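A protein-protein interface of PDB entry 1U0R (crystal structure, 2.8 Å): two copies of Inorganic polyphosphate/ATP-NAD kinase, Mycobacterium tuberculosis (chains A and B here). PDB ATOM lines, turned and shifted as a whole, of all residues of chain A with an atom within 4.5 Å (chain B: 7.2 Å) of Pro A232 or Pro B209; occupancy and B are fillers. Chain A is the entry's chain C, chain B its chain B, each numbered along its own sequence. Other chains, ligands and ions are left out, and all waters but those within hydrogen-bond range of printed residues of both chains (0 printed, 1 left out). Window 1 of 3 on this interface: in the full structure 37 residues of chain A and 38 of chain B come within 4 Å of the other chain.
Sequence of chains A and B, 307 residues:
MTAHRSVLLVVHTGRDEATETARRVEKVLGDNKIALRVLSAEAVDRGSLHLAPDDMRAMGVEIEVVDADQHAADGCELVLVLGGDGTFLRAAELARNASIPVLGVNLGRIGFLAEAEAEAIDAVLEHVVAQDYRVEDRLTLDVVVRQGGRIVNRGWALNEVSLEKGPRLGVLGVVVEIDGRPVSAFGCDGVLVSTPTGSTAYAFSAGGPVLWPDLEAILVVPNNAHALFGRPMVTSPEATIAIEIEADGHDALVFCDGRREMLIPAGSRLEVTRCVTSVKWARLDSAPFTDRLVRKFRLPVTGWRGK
Of the printed residues of chain B, Pro A232 touches Pro B209 (3.4 Å) and Val B210 (3.1 Å).
Of the printed residues of chain A, Pro B209 touches Pro A232.
Of the printed residues of chain B, Arg A231 touches Phe B204 (2.9 Å), Gly B207 (3.5 Å) and Gly B208 (2.8 Å).
Of the printed residues of chain A, Gly B207 touches Arg A231.
Printed residues of chain B within 4 Å of Val A234: Val B210 (2.8 Å), Leu B211 (3.3 Å) and Trp B212 (3.1 Å).
The nearest printed residue of chain A that does not touch Phe B204 is Pro A232 (7.1 Å).
The backbone carbonyl oxygen of Phe B204 lies within hydrogen-bond range of the guanidinium group of Arg A231, 2.9 Å away.
The backbone carbonyl oxygen (O) of Gly B208 is in hydrogen-bond range of the guanidinium group (NH1) of Arg A231 (2.8 Å).
The backbone NH (N) of Val B210 sits at hydrogen-bond distance from the backbone carbonyl oxygen (O) of Pro A232.
The backbone NH of Val A234 lies within hydrogen-bond range of the backbone carbonyl oxygen of Val B210 (2.8 Å).
N of Trp B212 lies within hydrogen-bond range of O of Val A234, 3.1 Å away.
The backbone carbonyl oxygen (O) of Gly A207 lies close to the guanidinium group (NH1) of Arg B231.
NH1 of Arg B231 lies within hydrogen-bond range of O of Gly A208 (2.7 Å).
N of Leu B211 lies within hydrogen-bond range of OG of Ser B199, 2.8 Å away.
O of Ala B203 sits at hydrogen-bond distance from N of Gly B208, 2.8 Å away.
The backbone NH of Val A220 sits at hydrogen-bond distance from the backbone carbonyl oxygen of Met A233 (2.8 Å).
Hydrophobic or aromatic side chains of chain B within 4 Å of the printed part of chain A: Phe B204, Pro B209, Val B210, Leu B211 and Trp B212.
Hydrophobic or aromatic side chains of chain A that line the printed part of chain B: Pro A209, Pro A232, Met A233 and Val A234.
Among the printed residues, 13 pairs touch across the chains.
Pro A209 touches Pro B232.
Arg A231 touches Gly B207 (NH1 to C, 3.5 Å).
O of Pro A232 touches CB of Pro B209, 3.4 Å away.
Val B210 touches Met A233 (O to CA, 3.3 Å).
Trp B212 touches Met A233 (CZ3 to CG, 3.3 Å).
O of Val A234 touches CA of Leu B211, 3.3 Å away.
Gly A207 touches Arg B231, and with the chains exchanged Arg A231 touches Gly B207.
Gly A208 touches Arg B231, and with the chains exchanged Arg A231 touches Gly B208.
Pro A209 touches Pro B232, and with the chains exchanged Pro A232 touches Pro B209.
Of the 13 pairs that touch across the chains among the printed residues, 6 have their exchanged pair printed and touching as well.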
ATOM      1  N   GLY A 207     -13.298   2.831  34.805  1.00  0.00           N
ATOM      2  CA  GLY A 207     -13.334   2.998  33.357  1.00  0.00           C
ATOM      3  C   GLY A 207     -12.147   2.480  32.567  1.00  0.00           C
ATOM      4  O   GLY A 207     -11.986   2.800  31.393  1.00  0.00           O
ATOM      5  N   GLY A 208     -11.334   1.652  33.200  1.00  0.00           N
ATOM      6  CA  GLY A 208     -10.049   1.296  32.646  1.00  0.00           C
ATOM      7  C   GLY A 208     -10.155   0.150  31.705  1.00  0.00           C
ATOM      8  O   GLY A 208     -11.132  -0.562  31.709  1.00  0.00           O
ATOM      9  N   PRO A 209      -9.160  -0.019  30.862  1.00  0.00           N
ATOM     10  CA  PRO A 209      -9.108  -1.164  29.947  1.00  0.00           C
ATOM     11  C   PRO A 209      -8.606  -2.418  30.615  1.00  0.00           C
ATOM     12  O   PRO A 209      -7.816  -2.316  31.559  1.00  0.00           O
ATOM     13  CB  PRO A 209      -8.089  -0.709  28.918  1.00  0.00           C
ATOM     14  CG  PRO A 209      -7.231   0.247  29.649  1.00  0.00           C
ATOM     15  CD  PRO A 209      -8.061   0.924  30.660  1.00  0.00           C
ATOM     16  N   LEU A 219      -0.706   1.347  34.027  1.00  0.00           N
ATOM     17  CA  LEU A 219      -1.971   1.909  33.601  1.00  0.00           C
ATOM     18  C   LEU A 219      -2.359   3.088  34.512  1.00  0.00           C
ATOM     19  O   LEU A 219      -2.206   2.994  35.715  1.00  0.00           O
ATOM     20  CB  LEU A 219      -3.009   0.809  33.644  1.00  0.00           C
ATOM     21  CG  LEU A 219      -4.488   1.125  33.592  1.00  0.00           C
ATOM     22  CD1 LEU A 219      -4.854   1.731  32.251  1.00  0.00           C
ATOM     23  CD2 LEU A 219      -5.184  -0.171  33.780  1.00  0.00           C
ATOM     24  N   VAL A 220      -2.822   4.196  33.929  1.00  0.00           N
ATOM     25  CA  VAL A 220      -3.342   5.316  34.686  1.00  0.00           C
ATOM     26  C   VAL A 220      -4.811   5.608  34.324  1.00  0.00           C
ATOM     27  O   VAL A 220      -5.162   5.800  33.179  1.00  0.00           O
ATOM     28  CB  VAL A 220      -2.560   6.541  34.404  1.00  0.00           C
ATOM     29  CG1 VAL A 220      -3.035   7.671  35.244  1.00  0.00           C
ATOM     30  CG2 VAL A 220      -1.155   6.310  34.703  1.00  0.00           C
ATOM     31  N   PRO A 222      -7.781   8.129  35.424  1.00  0.00           N
ATOM     32  CA  PRO A 222      -8.281   9.253  36.223  1.00  0.00           C
ATOM     33  C   PRO A 222      -9.566   8.806  36.869  1.00  0.00           C
ATOM     34  O   PRO A 222     -10.331   8.153  36.168  1.00  0.00           O
ATOM     35  CB  PRO A 222      -8.588  10.300  35.181  1.00  0.00           C
ATOM     36  CG  PRO A 222      -7.764   9.871  33.985  1.00  0.00           C
ATOM     37  CD  PRO A 222      -7.755   8.423  33.982  1.00  0.00           C
ATOM     38  N   GLY A 230     -10.189  12.438  30.197  1.00  0.00           N
ATOM     39  CA  GLY A 230      -9.825  11.582  31.300  1.00  0.00           C
ATOM     40  C   GLY A 230      -9.706  10.161  30.756  1.00  0.00           C
ATOM     41  O   GLY A 230     -10.188   9.216  31.393  1.00  0.00           O
ATOM     42  N   ARG A 231      -9.114   9.999  29.577  1.00  0.00           N
ATOM     43  CA  ARG A 231      -8.823   8.675  29.100  1.00  0.00           C
ATOM     44  C   ARG A 231      -7.801   7.956  29.963  1.00  0.00           C
ATOM     45  O   ARG A 231      -6.802   8.524  30.376  1.00  0.00           O
ATOM     46  CB  ARG A 231      -8.178   8.706  27.729  1.00  0.00           C
ATOM     47  CG  ARG A 231      -9.037   8.999  26.641  1.00  0.00           C
ATOM     48  CD  ARG A 231      -9.952   7.905  26.219  1.00  0.00           C
ATOM     49  NE  ARG A 231     -10.933   8.626  25.420  1.00  0.00           N
ATOM     50  CZ  ARG A 231     -11.111   8.494  24.132  1.00  0.00           C
ATOM     51  NH1 ARG A 231     -10.477   7.575  23.443  1.00  0.00           N
ATOM     52  NH2 ARG A 231     -11.970   9.280  23.547  1.00  0.00           N
ATOM     53  N   PRO A 232      -8.006   6.674  30.167  1.00  0.00           N
ATOM     54  CA  PRO A 232      -6.908   5.794  30.518  1.00  0.00           C
ATOM     55  C   PRO A 232      -5.653   6.051  29.642  1.00  0.00           C
ATOM     56  O   PRO A 232      -5.736   6.283  28.435  1.00  0.00           O
ATOM     57  CB  PRO A 232      -7.486   4.444  30.195  1.00  0.00           C
ATOM     58  CG  PRO A 232      -8.930   4.608  30.408  1.00  0.00           C
ATOM     59  CD  PRO A 232      -9.300   5.983  30.095  1.00  0.00           C
ATOM     60  N   MET A 233      -4.489   6.045  30.271  1.00  0.00           N
ATOM     61  CA  MET A 233      -3.223   6.110  29.574  1.00  0.00           C
ATOM     62  C   MET A 233      -2.500   4.822  29.966  1.00  0.00           C
ATOM     63  O   MET A 233      -2.665   4.335  31.090  1.00  0.00           O
ATOM     64  CB  MET A 233      -2.429   7.320  30.048  1.00  0.00           C
ATOM     65  CG  MET A 233      -2.937   8.710  29.595  1.00  0.00           C
ATOM     66  SD  MET A 233      -2.388   9.943  30.791  1.00  0.00           S
ATOM     67  CE  MET A 233      -3.527   9.751  32.112  1.00  0.00           C
ATOM     68  N   VAL A 234      -1.739   4.233  29.043  1.00  0.00           N
ATOM     69  CA  VAL A 234      -0.928   3.051  29.353  1.00  0.00           C
ATOM     70  C   VAL A 234       0.466   3.298  28.902  1.00  0.00           C
ATOM     71  O   VAL A 234       0.701   3.862  27.836  1.00  0.00           O
ATOM     72  CB  VAL A 234      -1.394   1.808  28.663  1.00  0.00           C
ATOM     73  CG1 VAL A 234      -0.555   0.633  29.112  1.00  0.00           C
ATOM     74  CG2 VAL A 234      -2.840   1.558  29.002  1.00  0.00           C
ATOM     75  N   PRO B 196       0.872   0.612  19.769  1.00  0.00           N
ATOM     76  CA  PRO B 196       0.921   1.825  20.590  1.00  0.00           C
ATOM     77  C   PRO B 196       1.084   3.136  19.809  1.00  0.00           C
ATOM     78  O   PRO B 196       0.648   4.210  20.244  1.00  0.00           O
ATOM     79  CB  PRO B 196       2.120   1.573  21.500  1.00  0.00           C
ATOM     80  CG  PRO B 196       2.150   0.093  21.637  1.00  0.00           C
ATOM     81  CD  PRO B 196       1.857  -0.381  20.239  1.00  0.00           C
ATOM     82  N   GLY B 198      -0.381   3.591  17.050  1.00  0.00           N
ATOM     83  CA  GLY B 198      -1.633   3.724  16.349  1.00  0.00           C
ATOM     84  C   GLY B 198      -2.749   3.977  17.296  1.00  0.00           C
ATOM     85  O   GLY B 198      -3.900   4.249  16.905  1.00  0.00           O
ATOM     86  N   SER B 199      -2.396   3.919  18.569  1.00  0.00           N
ATOM     87  CA  SER B 199      -3.366   3.982  19.653  1.00  0.00           C
ATOM     88  C   SER B 199      -3.905   5.392  19.772  1.00  0.00           C
ATOM     89  O   SER B 199      -4.754   5.677  20.599  1.00  0.00           O
ATOM     90  CB  SER B 199      -2.718   3.536  20.943  1.00  0.00           C
ATOM     91  OG  SER B 199      -2.277   4.659  21.626  1.00  0.00           O
ATOM     92  N   THR B 200      -3.464   6.230  18.867  1.00  0.00           N
ATOM     93  CA  THR B 200      -3.673   7.645  18.918  1.00  0.00           C
ATOM     94  C   THR B 200      -4.542   8.104  17.711  1.00  0.00           C
ATOM     95  O   THR B 200      -5.165   9.178  17.707  1.00  0.00           O
ATOM     96  CB  THR B 200      -2.250   8.210  18.900  1.00  0.00           C
ATOM     97  OG1 THR B 200      -2.095   9.151  19.966  1.00  0.00           O
ATOM     98  CG2 THR B 200      -1.902   8.914  17.609  1.00  0.00           C
ATOM     99  N   ALA B 203      -8.126   3.990  16.610  1.00  0.00           N
ATOM    100  CA  ALA B 203      -8.438   3.273  17.828  1.00  0.00           C
ATOM    101  C   ALA B 203      -8.730   4.275  18.902  1.00  0.00           C
ATOM    102  O   ALA B 203      -9.454   3.983  19.835  1.00  0.00           O
ATOM    103  CB  ALA B 203      -7.287   2.380  18.239  1.00  0.00           C
ATOM    104  N   PHE B 204      -8.157   5.465  18.801  1.00  0.00           N
ATOM    105  CA  PHE B 204      -8.461   6.441  19.823  1.00  0.00           C
ATOM    106  C   PHE B 204      -9.900   6.856  19.646  1.00  0.00           C
ATOM    107  O   PHE B 204     -10.605   6.961  20.639  1.00  0.00           O
ATOM    108  CB  PHE B 204      -7.542   7.635  19.785  1.00  0.00           C
ATOM    109  CG  PHE B 204      -7.991   8.770  20.670  1.00  0.00           C
ATOM    110  CD1 PHE B 204      -7.564   8.852  21.978  1.00  0.00           C
ATOM    111  CD2 PHE B 204      -8.819   9.762  20.183  1.00  0.00           C
ATOM    112  CE1 PHE B 204      -7.944   9.891  22.788  1.00  0.00           C
ATOM    113  CE2 PHE B 204      -9.230  10.797  20.979  1.00  0.00           C
ATOM    114  CZ  PHE B 204      -8.787  10.873  22.296  1.00  0.00           C
ATOM    115  N   GLY B 207     -12.525   4.876  20.846  1.00  0.00           N
ATOM    116  CA  GLY B 207     -12.670   4.965  22.279  1.00  0.00           C
ATOM    117  C   GLY B 207     -11.578   4.290  23.068  1.00  0.00           C
ATOM    118  O   GLY B 207     -11.688   4.076  24.255  1.00  0.00           O
ATOM    119  N   GLY B 208     -10.478   3.966  22.450  1.00  0.00           N
ATOM    120  CA  GLY B 208      -9.439   3.298  23.220  1.00  0.00           C
ATOM    121  C   GLY B 208      -8.591   4.233  24.044  1.00  0.00           C
ATOM    122  O   GLY B 208      -8.761   5.441  23.949  1.00  0.00           O
ATOM    123  N   PRO B 209      -7.673   3.669  24.836  1.00  0.00           N
ATOM    124  CA  PRO B 209      -6.812   4.432  25.738  1.00  0.00           C
ATOM    125  C   PRO B 209      -5.572   4.878  25.001  1.00  0.00           C
ATOM    126  O   PRO B 209      -5.366   4.383  23.889  1.00  0.00           O
ATOM    127  CB  PRO B 209      -6.451   3.398  26.767  1.00  0.00           C
ATOM    128  CG  PRO B 209      -6.393   2.132  25.979  1.00  0.00           C
ATOM    129  CD  PRO B 209      -7.406   2.225  24.917  1.00  0.00           C
ATOM    130  N   VAL B 210      -4.778   5.790  25.543  1.00  0.00           N
ATOM    131  CA  VAL B 210      -3.617   6.215  24.782  1.00  0.00           C
ATOM    132  C   VAL B 210      -2.401   5.499  25.307  1.00  0.00           C
ATOM    133  O   VAL B 210      -2.145   5.463  26.515  1.00  0.00           O
ATOM    134  CB  VAL B 210      -3.430   7.739  24.718  1.00  0.00           C
ATOM    135  CG1 VAL B 210      -4.091   8.434  25.879  1.00  0.00           C
ATOM    136  CG2 VAL B 210      -1.979   8.114  24.664  1.00  0.00           C
ATOM    137  N   LEU B 211      -1.659   4.898  24.388  1.00  0.00           N
ATOM    138  CA  LEU B 211      -0.484   4.129  24.736  1.00  0.00           C
ATOM    139  C   LEU B 211       0.691   4.944  24.328  1.00  0.00           C
ATOM    140  O   LEU B 211       0.748   5.323  23.170  1.00  0.00           O
ATOM    141  CB  LEU B 211      -0.478   2.800  23.977  1.00  0.00           C
ATOM    142  CG  LEU B 211      -1.241   1.663  24.668  1.00  0.00           C
ATOM    143  CD1 LEU B 211      -2.636   2.106  25.075  1.00  0.00           C
ATOM    144  CD2 LEU B 211      -1.333   0.452  23.788  1.00  0.00           C
ATOM    145  N   TRP B 212       1.612   5.234  25.257  1.00  0.00           N
ATOM    146  CA  TRP B 212       2.908   5.847  24.935  1.00  0.00           C
ATOM    147  C   TRP B 212       3.690   4.974  23.947  1.00  0.00           C
ATOM    148  O   TRP B 212       3.590   3.749  24.040  1.00  0.00           O
ATOM    149  CB  TRP B 212       3.685   6.082  26.212  1.00  0.00           C
ATOM    150  CG  TRP B 212       3.463   7.453  26.772  1.00  0.00           C
ATOM    151  CD1 TRP B 212       4.383   8.434  26.890  1.00  0.00           C
ATOM    152  CD2 TRP B 212       2.225   8.011  27.265  1.00  0.00           C
ATOM    153  NE1 TRP B 212       3.812   9.559  27.440  1.00  0.00           N
ATOM    154  CE2 TRP B 212       2.486   9.330  27.659  1.00  0.00           C
ATOM    155  CE3 TRP B 212       0.908   7.530  27.386  1.00  0.00           C
ATOM    156  CZ2 TRP B 212       1.505  10.159  28.180  1.00  0.00           C
ATOM    157  CZ3 TRP B 212      -0.070   8.363  27.920  1.00  0.00           C
ATOM    158  CH2 TRP B 212       0.228   9.647  28.312  1.00  0.00           C
ATOM    159  N   LEU B 219      -2.981  -3.589  21.163  1.00  0.00           N
ATOM    160  CA  LEU B 219      -4.209  -3.028  21.685  1.00  0.00           C
ATOM    161  C   LEU B 219      -5.395  -3.557  20.916  1.00  0.00           C
ATOM    162  O   LEU B 219      -5.347  -3.603  19.713  1.00  0.00           O
ATOM    163  CB  LEU B 219      -4.156  -1.517  21.578  1.00  0.00           C
ATOM    164  CG  LEU B 219      -5.302  -0.601  22.058  1.00  0.00           C
ATOM    165  CD1 LEU B 219      -5.917  -1.017  23.395  1.00  0.00           C
ATOM    166  CD2 LEU B 219      -4.808   0.802  22.163  1.00  0.00           C
ATOM    167  N   VAL B 220      -6.459  -3.980  21.589  1.00  0.00           N
ATOM    168  CA  VAL B 220      -7.697  -4.339  20.894  1.00  0.00           C
ATOM    169  C   VAL B 220      -8.841  -3.442  21.355  1.00  0.00           C
ATOM    170  O   VAL B 220      -9.144  -3.381  22.522  1.00  0.00           O
ATOM    171  CB  VAL B 220      -8.117  -5.780  21.160  1.00  0.00           C
ATOM    172  CG1 VAL B 220      -9.089  -6.230  20.110  1.00  0.00           C
ATOM    173  CG2 VAL B 220      -6.962  -6.682  21.133  1.00  0.00           C
ATOM    174  N   VAL B 221      -9.483  -2.762  20.427  1.00  0.00           N
ATOM    175  CA  VAL B 221     -10.613  -1.891  20.708  1.00  0.00           C
ATOM    176  C   VAL B 221     -11.794  -2.349  19.856  1.00  0.00           C
ATOM    177  O   VAL B 221     -11.778  -2.189  18.653  1.00  0.00           O
ATOM    178  CB  VAL B 221     -10.256  -0.461  20.337  1.00  0.00           C
ATOM    179  CG1 VAL B 221     -11.393   0.491  20.638  1.00  0.00           C
ATOM    180  CG2 VAL B 221      -9.012  -0.037  21.080  1.00  0.00           C
ATOM    181  N   ARG B 231     -15.008  -3.167  26.024  1.00  0.00           N
ATOM    182  CA  ARG B 231     -13.859  -2.501  26.587  1.00  0.00           C
ATOM    183  C   ARG B 231     -12.669  -2.855  25.781  1.00  0.00           C
ATOM    184  O   ARG B 231     -12.531  -4.017  25.357  1.00  0.00           O
ATOM    185  CB  ARG B 231     -13.605  -2.992  28.008  1.00  0.00           C
ATOM    186  CG  ARG B 231     -14.607  -2.521  28.947  1.00  0.00           C
ATOM    187  CD  ARG B 231     -14.208  -1.331  29.744  1.00  0.00           C
ATOM    188  NE  ARG B 231     -15.079  -1.353  30.894  1.00  0.00           N
ATOM    189  CZ  ARG B 231     -14.852  -0.756  32.010  1.00  0.00           C
ATOM    190  NH1 ARG B 231     -13.781  -0.003  32.161  1.00  0.00           N
ATOM    191  NH2 ARG B 231     -15.735  -0.866  32.977  1.00  0.00           N
ATOM    192  N   PRO B 232     -11.813  -1.863  25.555  1.00  0.00           N
ATOM    193  CA  PRO B 232     -10.512  -2.082  24.925  1.00  0.00           C
ATOM    194  C   PRO B 232      -9.700  -3.012  25.797  1.00  0.00           C
ATOM    195  O   PRO B 232      -9.910  -2.965  27.031  1.00  0.00           O
ATOM    196  CB  PRO B 232      -9.916  -0.688  24.899  1.00  0.00           C
ATOM    197  CG  PRO B 232     -11.082   0.158  24.833  1.00  0.00           C
ATOM    198  CD  PRO B 232     -12.057  -0.442  25.811  1.00  0.00           C
ATOM    199  N   MET B 233      -8.855  -3.856  25.182  1.00  0.00           N
ATOM    200  CA  MET B 233      -8.063  -4.845  25.893  1.00  0.00           C
ATOM    201  C   MET B 233      -6.628  -4.653  25.472  1.00  0.00           C
ATOM    202  O   MET B 233      -6.382  -4.270  24.322  1.00  0.00           O
ATOM    203  CB  MET B 233      -8.512  -6.240  25.535  1.00  0.00           C
ATOM    204  CG  MET B 233      -9.955  -6.639  26.009  1.00  0.00           C
ATOM    205  SD  MET B 233     -10.550  -8.066  25.041  1.00  0.00           S
ATOM    206  CE  MET B 233     -11.296  -7.142  23.826  1.00  0.00           C
ATOM    207  N   VAL B 234      -5.680  -4.869  26.396  1.00  0.00           N
ATOM    208  CA  VAL B 234      -4.255  -4.733  26.090  1.00  0.00           C
ATOM    209  C   VAL B 234      -3.390  -5.937  26.521  1.00  0.00           C
ATOM    210  O   VAL B 234      -3.594  -6.576  27.566  1.00  0.00           O
ATOM    211  CB  VAL B 234      -3.644  -3.477  26.665  1.00  0.00           C
ATOM    212  CG1 VAL B 234      -2.400  -3.137  25.909  1.00  0.00           C
ATOM    213  CG2 VAL B 234      -4.589  -2.352  26.552  1.00  0.00           C
